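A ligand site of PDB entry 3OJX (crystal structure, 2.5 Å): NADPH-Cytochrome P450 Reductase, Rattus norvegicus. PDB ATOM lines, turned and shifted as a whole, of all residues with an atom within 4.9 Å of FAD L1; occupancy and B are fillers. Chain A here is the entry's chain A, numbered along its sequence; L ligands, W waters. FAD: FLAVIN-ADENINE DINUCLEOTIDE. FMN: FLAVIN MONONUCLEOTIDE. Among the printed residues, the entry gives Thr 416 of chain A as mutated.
N of Val 420 lies within hydrogen-bond range of OG1 of Thr 435 (3.1 Å).
NE1 of Trp 621 is in hydrogen-bond range of OG of Ser 401.
OG of Ser 401 lies within hydrogen-bond range of OD2 of Asp 619 (3.1 Å).
The indole nitrogen (NE1) of Trp 621 sits at hydrogen-bond distance from the side-chain carboxylate (OD2) of Asp 619 (3.1 Å).
The backbone NH (N) of Gly 432 is in hydrogen-bond range of the backbone carbonyl oxygen (O) of Val 420, 3.0 Å away.
O of Gly 432 lies within hydrogen-bond range of OG of Ser 436 (3.0 Å).
The side-chain hydroxyl (OH) of Tyr 422 sits at hydrogen-bond distance from the guanidinium group (NE) of Arg 368, at 3.5 Å.
NE2 of His 263 is in hydrogen-bond range of OD1 of Asp 619, 3.0 Å away.
N of Tyr 399 lies within hydrogen-bond range of O2' of FAD L1 (3.4 Å).
O of Tyr 399 lies within hydrogen-bond range of O2' of FAD L1, at 2.6 Å.
An oxygen (O2P) of FAD L1 lies within hydrogen-bond range of the backbone NH of Thr 435, at 3.0 Å.
The side-chain hydroxyl (OG1) of Thr 435 lies within hydrogen-bond range of an oxygen (O2P) of FAD L1 (2.8 Å).
The backbone carbonyl oxygen (O) of Thr 416 sits at hydrogen-bond distance from a nitrogen (N3) of FAD L1 (2.8 Å).
An oxygen (O1P) of FAD L1 lies within hydrogen-bond range of the backbone NH of Ala 434 (2.8 Å).
An oxygen (O1A) of FAD L1 lies within hydrogen-bond range of the backbone NH (N) of Val 433 (2.9 Å).
The side-chain hydroxyl (OH) of Tyr 400 sits at hydrogen-bond distance from an oxygen (O4') of FAD L1 (3.0 Å).
NE of Arg 398 is in salt-bridge range of O1P of FAD L1, at 3.0 Å.
An oxygen (O4) of FAD L1 sits at hydrogen-bond distance from the backbone NH (N) of Ser 401, at 3.0 Å.
A nitrogen (N5) of FAD L1 lies close to the indole nitrogen (NE1) of Trp 621 (3.5 Å).
An oxygen (O2B) of FAD L1 sits at hydrogen-bond distance from the guanidinium group (NH2) of Arg 368, 3.3 Å away.
The backbone NH of Val 418 lies within hydrogen-bond range of an oxygen (O2) of FAD L1 (3.4 Å).
The backbone NH of Gln 31 lies within hydrogen-bond range of an oxygen (O2P) of FMN L2, at 2.9 Å.
Water W1 lies within hydrogen-bond range of O4B of FAD L1 and OH of Tyr 422.
Water W2 bridges an oxygen (O2') of FAD L1 (2.8 Å) and the backbone NH (N) of Tyr 399 (2.8 Å).
Water W4 lies within hydrogen-bond range of the backbone NH of Thr 416, the backbone carbonyl oxygen of Ser 401 and an oxygen (O4) of FAD L1.
Residues that only touch FAD L1: His 263, Ala 417, Val 420, Tyr 422, Gly 432, Ala 482 and Val 620.
Hydrophobic or aromatic side chains that line FAD L1: His 263, Tyr 400, Ala 417, Val 418, Val 420, Tyr 422, Val 433, Ala 434, Ala 482 and Trp 621.
18 residues have an atom within 4 Å of FAD L1: His 263, Arg 368, Arg 398, Tyr 399, Tyr 400, Ser 401, Thr 416, Ala 417, Val 418, Val 420, Tyr 422, Gly 432, Val 433, Ala 434, Thr 435, Ala 482, Val 620 and Trp 621.
The nearest printed residue that does not touch FAD L1 is Lys 431 (4.1 Å).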
ATOM      1  N   GLN A  31      -2.335 -17.115  -0.535  1.00  0.00           N
ATOM      2  CA  GLN A  31      -1.086 -16.457  -0.185  1.00  0.00           C
ATOM      3  C   GLN A  31      -1.232 -15.552   1.055  1.00  0.00           C
ATOM      4  O   GLN A  31      -0.247 -15.307   1.750  1.00  0.00           O
ATOM      5  CB  GLN A  31      -0.573 -15.644  -1.401  1.00  0.00           C
ATOM      6  CG  GLN A  31       0.952 -15.465  -1.398  1.00  0.00           C
ATOM      7  CD  GLN A  31       1.505 -14.880  -2.712  1.00  0.00           C
ATOM      8  OE1 GLN A  31       1.442 -15.512  -3.776  1.00  0.00           O
ATOM      9  NE2 GLN A  31       2.064 -13.687  -2.616  1.00  0.00           N
ATOM     10  N   HIS A 263      11.123 -14.197  -5.321  1.00  0.00           N
ATOM     11  CA  HIS A 263      10.713 -13.526  -4.099  1.00  0.00           C
ATOM     12  C   HIS A 263      11.197 -14.306  -2.886  1.00  0.00           C
ATOM     13  O   HIS A 263      11.397 -15.518  -2.957  1.00  0.00           O
ATOM     14  CB  HIS A 263       9.189 -13.402  -4.048  1.00  0.00           C
ATOM     15  CG  HIS A 263       8.620 -12.597  -5.179  1.00  0.00           C
ATOM     16  ND1 HIS A 263       7.827 -13.162  -6.155  1.00  0.00           N
ATOM     17  CD2 HIS A 263       8.704 -11.281  -5.469  1.00  0.00           C
ATOM     18  CE1 HIS A 263       7.456 -12.225  -7.009  1.00  0.00           C
ATOM     19  NE2 HIS A 263       7.981 -11.071  -6.618  1.00  0.00           N
ATOM     20  N   THR A 322      -3.025  -7.219  13.780  1.00  0.00           N
ATOM     21  CA  THR A 322      -2.930  -5.854  13.278  1.00  0.00           C
ATOM     22  C   THR A 322      -3.902  -5.483  12.159  1.00  0.00           C
ATOM     23  O   THR A 322      -4.167  -4.312  11.937  1.00  0.00           O
ATOM     24  CB  THR A 322      -1.522  -5.540  12.805  1.00  0.00           C
ATOM     25  OG1 THR A 322      -1.091  -6.563  11.902  1.00  0.00           O
ATOM     26  CG2 THR A 322      -0.575  -5.466  13.971  1.00  0.00           C
ATOM     27  N   ARG A 368      -8.748   1.532   9.598  1.00  0.00           N
ATOM     28  CA  ARG A 368      -7.700   0.581   9.928  1.00  0.00           C
ATOM     29  C   ARG A 368      -7.581   0.232  11.399  1.00  0.00           C
ATOM     30  O   ARG A 368      -6.484   0.203  11.954  1.00  0.00           O
ATOM     31  CB  ARG A 368      -6.337   1.084   9.409  1.00  0.00           C
ATOM     32  CG  ARG A 368      -6.227   1.177   7.872  1.00  0.00           C
ATOM     33  CD  ARG A 368      -6.293  -0.180   7.165  1.00  0.00           C
ATOM     34  NE  ARG A 368      -5.300  -1.123   7.684  1.00  0.00           N
ATOM     35  CZ  ARG A 368      -5.091  -2.338   7.183  1.00  0.00           C
ATOM     36  NH1 ARG A 368      -4.155  -3.128   7.718  1.00  0.00           N
ATOM     37  NH2 ARG A 368      -5.816  -2.773   6.157  1.00  0.00           N
ATOM     38  N   ARG A 398       5.417 -12.357   4.673  1.00  0.00           N
ATOM     39  CA  ARG A 398       5.449 -11.157   3.837  1.00  0.00           C
ATOM     40  C   ARG A 398       6.440 -11.417   2.701  1.00  0.00           C
ATOM     41  O   ARG A 398       7.534 -11.937   2.935  1.00  0.00           O
ATOM     42  CB  ARG A 398       5.881  -9.940   4.650  1.00  0.00           C
ATOM     43  CG  ARG A 398       4.725  -9.137   5.253  1.00  0.00           C
ATOM     44  CD  ARG A 398       3.860  -9.949   6.201  1.00  0.00           C
ATOM     45  NE  ARG A 398       2.845  -9.111   6.835  1.00  0.00           N
ATOM     46  CZ  ARG A 398       1.910  -9.538   7.682  1.00  0.00           C
ATOM     47  NH1 ARG A 398       1.039  -8.675   8.196  1.00  0.00           N
ATOM     48  NH2 ARG A 398       1.857 -10.818   8.032  1.00  0.00           N
ATOM     49  N   TYR A 399       6.065 -11.072   1.485  1.00  0.00           N
ATOM     50  CA  TYR A 399       6.926 -11.305   0.329  1.00  0.00           C
ATOM     51  C   TYR A 399       7.701 -10.071  -0.119  1.00  0.00           C
ATOM     52  O   TYR A 399       7.178  -8.950  -0.113  1.00  0.00           O
ATOM     53  CB  TYR A 399       6.093 -11.844  -0.828  1.00  0.00           C
ATOM     54  CG  TYR A 399       5.539 -13.221  -0.574  1.00  0.00           C
ATOM     55  CD1 TYR A 399       6.082 -14.336  -1.220  1.00  0.00           C
ATOM     56  CD2 TYR A 399       4.502 -13.435   0.330  1.00  0.00           C
ATOM     57  CE1 TYR A 399       5.596 -15.617  -0.980  1.00  0.00           C
ATOM     58  CE2 TYR A 399       4.009 -14.704   0.571  1.00  0.00           C
ATOM     59  CZ  TYR A 399       4.559 -15.789  -0.080  1.00  0.00           C
ATOM     60  OH  TYR A 399       4.085 -17.064   0.155  1.00  0.00           O
ATOM     61  N   TYR A 400       8.954 -10.313  -0.518  1.00  0.00           N
ATOM     62  CA  TYR A 400       9.849  -9.247  -0.981  1.00  0.00           C
ATOM     63  C   TYR A 400      10.602  -9.692  -2.234  1.00  0.00           C
ATOM     64  O   TYR A 400      11.004 -10.860  -2.363  1.00  0.00           O
ATOM     65  CB  TYR A 400      10.827  -8.908   0.135  1.00  0.00           C
ATOM     66  CG  TYR A 400      10.118  -8.317   1.325  1.00  0.00           C
ATOM     67  CD1 TYR A 400       9.821  -6.956   1.394  1.00  0.00           C
ATOM     68  CD2 TYR A 400       9.634  -9.144   2.339  1.00  0.00           C
ATOM     69  CE1 TYR A 400       9.064  -6.426   2.426  1.00  0.00           C
ATOM     70  CE2 TYR A 400       8.866  -8.630   3.388  1.00  0.00           C
ATOM     71  CZ  TYR A 400       8.573  -7.278   3.414  1.00  0.00           C
ATOM     72  OH  TYR A 400       7.755  -6.786   4.397  1.00  0.00           O
ATOM     73  N   SER A 401      10.775  -8.769  -3.189  1.00  0.00           N
ATOM     74  CA  SER A 401      11.489  -9.076  -4.422  1.00  0.00           C
ATOM     75  C   SER A 401      12.996  -9.098  -4.188  1.00  0.00           C
ATOM     76  O   SER A 401      13.610  -8.067  -3.946  1.00  0.00           O
ATOM     77  CB  SER A 401      11.155  -8.032  -5.493  1.00  0.00           C
ATOM     78  OG  SER A 401       9.776  -8.059  -5.821  1.00  0.00           O
ATOM     79  N   THR A 416      15.006  -4.997  -0.441  1.00  0.00           N
ATOM     80  CA  THR A 416      14.860  -3.534  -0.471  1.00  0.00           C
ATOM     81  C   THR A 416      13.448  -3.262   0.047  1.00  0.00           C
ATOM     82  O   THR A 416      12.484  -3.715  -0.558  1.00  0.00           O
ATOM     83  CB  THR A 416      14.979  -2.952  -1.903  1.00  0.00           C
ATOM     84  OG1 THR A 416      16.211  -3.356  -2.513  1.00  0.00           O
ATOM     85  CG2 THR A 416      14.935  -1.424  -1.849  1.00  0.00           C
ATOM     86  N   ALA A 417      13.326  -2.535   1.159  1.00  0.00           N
ATOM     87  CA  ALA A 417      12.002  -2.298   1.712  1.00  0.00           C
ATOM     88  C   ALA A 417      11.799  -0.957   2.380  1.00  0.00           C
ATOM     89  O   ALA A 417      12.740  -0.371   2.894  1.00  0.00           O
ATOM     90  CB  ALA A 417      11.672  -3.377   2.698  1.00  0.00           C
ATOM     91  N   VAL A 418      10.553  -0.494   2.368  1.00  0.00           N
ATOM     92  CA  VAL A 418      10.178   0.764   2.990  1.00  0.00           C
ATOM     93  C   VAL A 418       9.410   0.413   4.271  1.00  0.00           C
ATOM     94  O   VAL A 418       8.435  -0.326   4.224  1.00  0.00           O
ATOM     95  CB  VAL A 418       9.265   1.596   2.056  1.00  0.00           C
ATOM     96  CG1 VAL A 418       8.074   0.768   1.606  1.00  0.00           C
ATOM     97  CG2 VAL A 418       8.803   2.847   2.754  1.00  0.00           C
ATOM     98  N   VAL A 420       6.805   0.491   7.053  1.00  0.00           N
ATOM     99  CA  VAL A 420       5.442   0.980   7.027  1.00  0.00           C
ATOM    100  C   VAL A 420       5.040   1.511   8.400  1.00  0.00           C
ATOM    101  O   VAL A 420       5.163   0.819   9.404  1.00  0.00           O
ATOM    102  CB  VAL A 420       4.471  -0.141   6.582  1.00  0.00           C
ATOM    103  CG1 VAL A 420       3.047   0.365   6.619  1.00  0.00           C
ATOM    104  CG2 VAL A 420       4.827  -0.605   5.175  1.00  0.00           C
ATOM    105  N   TYR A 422       2.099   4.717   9.685  1.00  0.00           N
ATOM    106  CA  TYR A 422       1.256   5.847   9.347  1.00  0.00           C
ATOM    107  C   TYR A 422       0.258   6.132  10.440  1.00  0.00           C
ATOM    108  O   TYR A 422       0.126   5.353  11.385  1.00  0.00           O
ATOM    109  CB  TYR A 422       0.496   5.530   8.075  1.00  0.00           C
ATOM    110  CG  TYR A 422      -0.302   4.258   8.192  1.00  0.00           C
ATOM    111  CD1 TYR A 422       0.299   3.007   8.043  1.00  0.00           C
ATOM    112  CD2 TYR A 422      -1.673   4.284   8.465  1.00  0.00           C
ATOM    113  CE1 TYR A 422      -0.435   1.826   8.171  1.00  0.00           C
ATOM    114  CE2 TYR A 422      -2.414   3.115   8.594  1.00  0.00           C
ATOM    115  CZ  TYR A 422      -1.794   1.891   8.446  1.00  0.00           C
ATOM    116  OH  TYR A 422      -2.531   0.750   8.559  1.00  0.00           O
ATOM    117  N   LYS A 431       1.705   0.271  12.704  1.00  0.00           N
ATOM    118  CA  LYS A 431       3.051  -0.153  12.290  1.00  0.00           C
ATOM    119  C   LYS A 431       2.922  -1.421  11.479  1.00  0.00           C
ATOM    120  O   LYS A 431       2.083  -2.271  11.780  1.00  0.00           O
ATOM    121  CB  LYS A 431       3.925  -0.426  13.520  1.00  0.00           C
ATOM    122  CG  LYS A 431       4.129   0.779  14.418  1.00  0.00           C
ATOM    123  CD  LYS A 431       5.210   1.698  13.860  1.00  0.00           C
ATOM    124  CE  LYS A 431       6.576   1.034  13.958  1.00  0.00           C
ATOM    125  NZ  LYS A 431       6.902   0.667  15.376  1.00  0.00           N
ATOM    126  N   GLY A 432       3.743  -1.558  10.445  1.00  0.00           N
ATOM    127  CA  GLY A 432       3.700  -2.753   9.626  1.00  0.00           C
ATOM    128  C   GLY A 432       4.427  -3.849  10.377  1.00  0.00           C
ATOM    129  O   GLY A 432       5.460  -3.602  10.980  1.00  0.00           O
ATOM    130  N   VAL A 433       3.906  -5.074  10.325  1.00  0.00           N
ATOM    131  CA  VAL A 433       4.535  -6.172  11.048  1.00  0.00           C
ATOM    132  C   VAL A 433       5.910  -6.588  10.549  1.00  0.00           C
ATOM    133  O   VAL A 433       6.901  -6.456  11.264  1.00  0.00           O
ATOM    134  CB  VAL A 433       3.628  -7.415  11.074  1.00  0.00           C
ATOM    135  CG1 VAL A 433       4.294  -8.508  11.869  1.00  0.00           C
ATOM    136  CG2 VAL A 433       2.270  -7.065  11.682  1.00  0.00           C
ATOM    137  N   ALA A 434       5.996  -7.089   9.319  1.00  0.00           N
ATOM    138  CA  ALA A 434       7.274  -7.532   8.783  1.00  0.00           C
ATOM    139  C   ALA A 434       8.346  -6.441   8.767  1.00  0.00           C
ATOM    140  O   ALA A 434       9.455  -6.652   9.262  1.00  0.00           O
ATOM    141  CB  ALA A 434       7.082  -8.114   7.386  1.00  0.00           C
ATOM    142  N   THR A 435       8.040  -5.276   8.197  1.00  0.00           N
ATOM    143  CA  THR A 435       9.033  -4.190   8.113  1.00  0.00           C
ATOM    144  C   THR A 435       9.515  -3.637   9.451  1.00  0.00           C
ATOM    145  O   THR A 435      10.683  -3.258   9.551  1.00  0.00           O
ATOM    146  CB  THR A 435       8.521  -3.013   7.242  1.00  0.00           C
ATOM    147  OG1 THR A 435       7.369  -2.410   7.844  1.00  0.00           O
ATOM    148  CG2 THR A 435       8.171  -3.496   5.839  1.00  0.00           C
ATOM    149  N   SER A 436       8.652  -3.577  10.465  1.00  0.00           N
ATOM    150  CA  SER A 436       9.069  -3.074  11.789  1.00  0.00           C
ATOM    151  C   SER A 436      10.030  -4.084  12.403  1.00  0.00           C
ATOM    152  O   SER A 436      11.073  -3.722  12.968  1.00  0.00           O
ATOM    153  CB  SER A 436       7.874  -2.899  12.720  1.00  0.00           C
ATOM    154  OG  SER A 436       7.196  -1.686  12.473  1.00  0.00           O
ATOM    155  N   THR A 479      10.781   1.723  -4.395  1.00  0.00           N
ATOM    156  CA  THR A 479      11.427   0.490  -3.963  1.00  0.00           C
ATOM    157  C   THR A 479      11.220  -0.596  -5.011  1.00  0.00           C
ATOM    158  O   THR A 479      11.881  -1.628  -4.981  1.00  0.00           O
ATOM    159  CB  THR A 479      10.860   0.000  -2.612  1.00  0.00           C
ATOM    160  OG1 THR A 479       9.590  -0.618  -2.831  1.00  0.00           O
ATOM    161  CG2 THR A 479      10.672   1.184  -1.654  1.00  0.00           C
ATOM    162  N   ALA A 482      13.912  -2.780  -6.625  1.00  0.00           N
ATOM    163  CA  ALA A 482      14.479  -3.968  -6.009  1.00  0.00           C
ATOM    164  C   ALA A 482      14.890  -5.105  -6.935  1.00  0.00           C
ATOM    165  O   ALA A 482      16.067  -5.435  -7.019  1.00  0.00           O
ATOM    166  CB  ALA A 482      13.539  -4.494  -4.925  1.00  0.00           C
ATOM    167  N   ASP A 619       5.669  -7.563 -12.401  1.00  0.00           N
ATOM    168  CA  ASP A 619       5.769  -8.121 -11.061  1.00  0.00           C
ATOM    169  C   ASP A 619       4.963  -7.173 -10.195  1.00  0.00           C
ATOM    170  O   ASP A 619       5.452  -6.112  -9.792  1.00  0.00           O
ATOM    171  CB  ASP A 619       7.218  -8.175 -10.578  1.00  0.00           C
ATOM    172  CG  ASP A 619       7.369  -8.929  -9.268  1.00  0.00           C
ATOM    173  OD1 ASP A 619       6.822 -10.050  -9.194  1.00  0.00           O
ATOM    174  OD2 ASP A 619       8.030  -8.424  -8.334  1.00  0.00           O
ATOM    175  N   VAL A 620       3.722  -7.554  -9.915  1.00  0.00           N
ATOM    176  CA  VAL A 620       2.826  -6.705  -9.134  1.00  0.00           C
ATOM    177  C   VAL A 620       2.844  -6.927  -7.619  1.00  0.00           C
ATOM    178  O   VAL A 620       2.707  -8.046  -7.138  1.00  0.00           O
ATOM    179  CB  VAL A 620       1.375  -6.822  -9.694  1.00  0.00           C
ATOM    180  CG1 VAL A 620       1.306  -7.957 -10.713  1.00  0.00           C
ATOM    181  CG2 VAL A 620       0.379  -7.034  -8.570  1.00  0.00           C
ATOM    182  N   TRP A 621       3.023  -5.834  -6.893  1.00  0.00           N
ATOM    183  CA  TRP A 621       3.081  -5.867  -5.434  1.00  0.00           C
ATOM    184  C   TRP A 621       1.737  -5.562  -4.773  1.00  0.00           C
ATOM    185  O   TRP A 621       1.524  -5.857  -3.593  1.00  0.00           O
ATOM    186  CB  TRP A 621       4.141  -4.863  -4.944  1.00  0.00           C
ATOM    187  CG  TRP A 621       5.542  -5.220  -5.320  1.00  0.00           C
ATOM    188  CD1 TRP A 621       5.939  -6.246  -6.125  1.00  0.00           C
ATOM    189  CD2 TRP A 621       6.726  -4.519  -4.940  1.00  0.00           C
ATOM    190  NE1 TRP A 621       7.311  -6.236  -6.263  1.00  0.00           N
ATOM    191  CE2 TRP A 621       7.816  -5.180  -5.544  1.00  0.00           C
ATOM    192  CE3 TRP A 621       6.982  -3.390  -4.149  1.00  0.00           C
ATOM    193  CZ2 TRP A 621       9.140  -4.745  -5.390  1.00  0.00           C
ATOM    194  CZ3 TRP A 621       8.295  -2.961  -3.989  1.00  0.00           C
ATOM    195  CH2 TRP A 621       9.355  -3.638  -4.603  1.00  0.00           C
HETATM  196  PA  FAD L   1       1.551  -4.832   7.274  1.00  0.00           P
HETATM  197  O1A FAD L   1       1.517  -4.884   8.737  1.00  0.00           O
HETATM  198  O2A FAD L   1       1.282  -6.085   6.587  1.00  0.00           O
HETATM  199  O5B FAD L   1       0.514  -3.717   6.730  1.00  0.00           O
HETATM  200  C5B FAD L   1       0.313  -3.411   5.316  1.00  0.00           C
HETATM  201  C4B FAD L   1      -1.076  -2.811   5.073  1.00  0.00           C
HETATM  202  O4B FAD L   1      -1.220  -1.558   5.740  1.00  0.00           O
HETATM  203  C3B FAD L   1      -1.366  -2.484   3.603  1.00  0.00           C
HETATM  204  O3B FAD L   1      -1.756  -3.644   2.865  1.00  0.00           O
HETATM  205  C2B FAD L   1      -2.460  -1.419   3.695  1.00  0.00           C
HETATM  206  O2B FAD L   1      -3.794  -1.960   3.737  1.00  0.00           O
HETATM  207  C1B FAD L   1      -2.069  -0.690   4.961  1.00  0.00           C
HETATM  208  N9A FAD L   1      -1.351   0.614   4.805  1.00  0.00           N
HETATM  209  C8A FAD L   1      -0.040   0.949   4.483  1.00  0.00           C
HETATM  210  N7A FAD L   1       0.321   2.274   4.423  1.00  0.00           N
HETATM  211  C5A FAD L   1      -0.921   2.831   4.731  1.00  0.00           C
HETATM  212  C6A FAD L   1      -1.381   4.193   4.870  1.00  0.00           C
HETATM  213  N6A FAD L   1      -0.580   5.245   4.700  1.00  0.00           N
HETATM  214  N1A FAD L   1      -2.729   4.445   5.206  1.00  0.00           N
HETATM  215  C2A FAD L   1      -3.638   3.404   5.403  1.00  0.00           C
HETATM  216  N3A FAD L   1      -3.331   2.066   5.307  1.00  0.00           N
HETATM  217  C4A FAD L   1      -1.946   1.835   4.966  1.00  0.00           C
HETATM  218  N1  FAD L   1       7.551  -4.408  -0.246  1.00  0.00           N
HETATM  219  C2  FAD L   1       8.788  -3.825  -0.193  1.00  0.00           C
HETATM  220  O2  FAD L   1       8.973  -2.898   0.603  1.00  0.00           O
HETATM  221  N3  FAD L   1       9.771  -4.358  -1.072  1.00  0.00           N
HETATM  222  C4  FAD L   1       9.595  -5.429  -2.005  1.00  0.00           C
HETATM  223  O4  FAD L   1      10.538  -5.782  -2.707  1.00  0.00           O
HETATM  224  C4X FAD L   1       8.239  -6.008  -2.025  1.00  0.00           C
HETATM  225  N5  FAD L   1       7.990  -7.058  -2.935  1.00  0.00           N
HETATM  226  C5X FAD L   1       6.684  -7.617  -2.954  1.00  0.00           C
HETATM  227  C6  FAD L   1       6.454  -8.701  -3.909  1.00  0.00           C
HETATM  228  C7  FAD L   1       5.175  -9.355  -4.057  1.00  0.00           C
HETATM  229  C7M FAD L   1       4.987 -10.482  -5.076  1.00  0.00           C
HETATM  230  C8  FAD L   1       4.043  -8.875  -3.150  1.00  0.00           C
HETATM  231  C8M FAD L   1       2.617  -9.474  -3.196  1.00  0.00           C
HETATM  232  C9  FAD L   1       4.257  -7.846  -2.226  1.00  0.00           C
HETATM  233  C9A FAD L   1       5.547  -7.186  -2.083  1.00  0.00           C
HETATM  234  N10 FAD L   1       5.866  -6.084  -1.141  1.00  0.00           N
HETATM  235  C10 FAD L   1       7.250  -5.458  -1.114  1.00  0.00           C
HETATM  236  C1' FAD L   1       4.915  -5.496  -0.151  1.00  0.00           C
HETATM  237  C2' FAD L   1       5.408  -6.471   1.036  1.00  0.00           C
HETATM  238  O2' FAD L   1       5.069  -7.876   0.873  1.00  0.00           O
HETATM  239  C3' FAD L   1       4.826  -5.999   2.418  1.00  0.00           C
HETATM  240  O3' FAD L   1       3.409  -6.055   2.267  1.00  0.00           O
HETATM  241  C4' FAD L   1       5.095  -4.548   2.891  1.00  0.00           C
HETATM  242  O4' FAD L   1       6.495  -4.468   3.035  1.00  0.00           O
HETATM  243  C5' FAD L   1       4.483  -4.215   4.277  1.00  0.00           C
HETATM  244  O5' FAD L   1       4.408  -5.281   5.157  1.00  0.00           O
HETATM  245  P   FAD L   1       4.260  -5.079   6.708  1.00  0.00           P
HETATM  246  O1P FAD L   1       4.162  -6.458   7.246  1.00  0.00           O
HETATM  247  O2P FAD L   1       5.391  -4.269   7.257  1.00  0.00           O
HETATM  248  O3P FAD L   1       2.925  -4.308   6.770  1.00  0.00           O
HETATM  249  N1  FMN L   2      -7.433 -11.009  -8.437  1.00  0.00           N
HETATM  250  C2  FMN L   2      -7.696 -11.315  -9.742  1.00  0.00           C
HETATM  251  O2  FMN L   2      -8.794 -11.719 -10.100  1.00  0.00           O
HETATM  252  N3  FMN L   2      -6.670 -11.131 -10.650  1.00  0.00           N
HETATM  253  C4  FMN L   2      -5.377 -10.676 -10.379  1.00  0.00           C
HETATM  254  O4  FMN L   2      -4.646 -10.615 -11.369  1.00  0.00           O
HETATM  255  C4A FMN L   2      -5.073 -10.360  -9.026  1.00  0.00           C
HETATM  256  N5  FMN L   2      -3.783  -9.900  -8.733  1.00  0.00           N
HETATM  257  C5A FMN L   2      -3.563  -9.597  -7.391  1.00  0.00           C
HETATM  258  C6  FMN L   2      -2.245  -9.116  -7.067  1.00  0.00           C
HETATM  259  C7  FMN L   2      -1.895  -8.773  -5.734  1.00  0.00           C
HETATM  260  C7M FMN L   2      -0.446  -8.273  -5.525  1.00  0.00           C
HETATM  261  C8  FMN L   2      -2.880  -8.896  -4.623  1.00  0.00           C
HETATM  262  C8M FMN L   2      -2.655  -8.588  -3.305  1.00  0.00           C
HETATM  263  C9  FMN L   2      -4.151  -9.343  -4.935  1.00  0.00           C
HETATM  264  C9A FMN L   2      -4.530  -9.717  -6.297  1.00  0.00           C
HETATM  265  N10 FMN L   2      -5.874 -10.213  -6.684  1.00  0.00           N
HETATM  266  C10 FMN L   2      -6.159 -10.546  -8.096  1.00  0.00           C
HETATM  267  C1' FMN L   2      -6.889 -10.360  -5.678  1.00  0.00           C
HETATM  268  C2' FMN L   2      -6.783 -11.645  -4.840  1.00  0.00           C
HETATM  269  O2' FMN L   2      -6.911 -12.789  -5.761  1.00  0.00           O
HETATM  270  C3' FMN L   2      -7.879 -11.653  -3.808  1.00  0.00           C
HETATM  271  O3' FMN L   2      -7.632 -10.500  -2.963  1.00  0.00           O
HETATM  272  C4' FMN L   2      -7.785 -12.992  -2.992  1.00  0.00           C
HETATM  273  O4' FMN L   2      -8.757 -12.854  -2.246  1.00  0.00           O
HETATM  274  C5' FMN L   2      -6.576 -13.137  -2.091  1.00  0.00           C
HETATM  275  O5' FMN L   2      -6.601 -14.460  -1.447  1.00  0.00           O
HETATM  276  P   FMN L   2      -5.588 -15.085  -0.401  1.00  0.00           P
HETATM  277  O1P FMN L   2      -5.727 -14.418   0.915  1.00  0.00           O
HETATM  278  O2P FMN L   2      -4.216 -15.058  -1.151  1.00  0.00           O
HETATM  279  O3P FMN L   2      -6.241 -16.541  -0.242  1.00  0.00           O
HETATM  280  O   HOH W   1      -0.893  -1.551   8.434  1.00  0.00           O
HETATM  281  O   HOH W   2       3.470 -10.102   1.236  1.00  0.00           O
HETATM  282  O   HOH W   3       1.440  -7.203   4.157  1.00  0.00           O
HETATM  283  O   HOH W   4      13.177  -6.662  -1.617  1.00  0.00           O
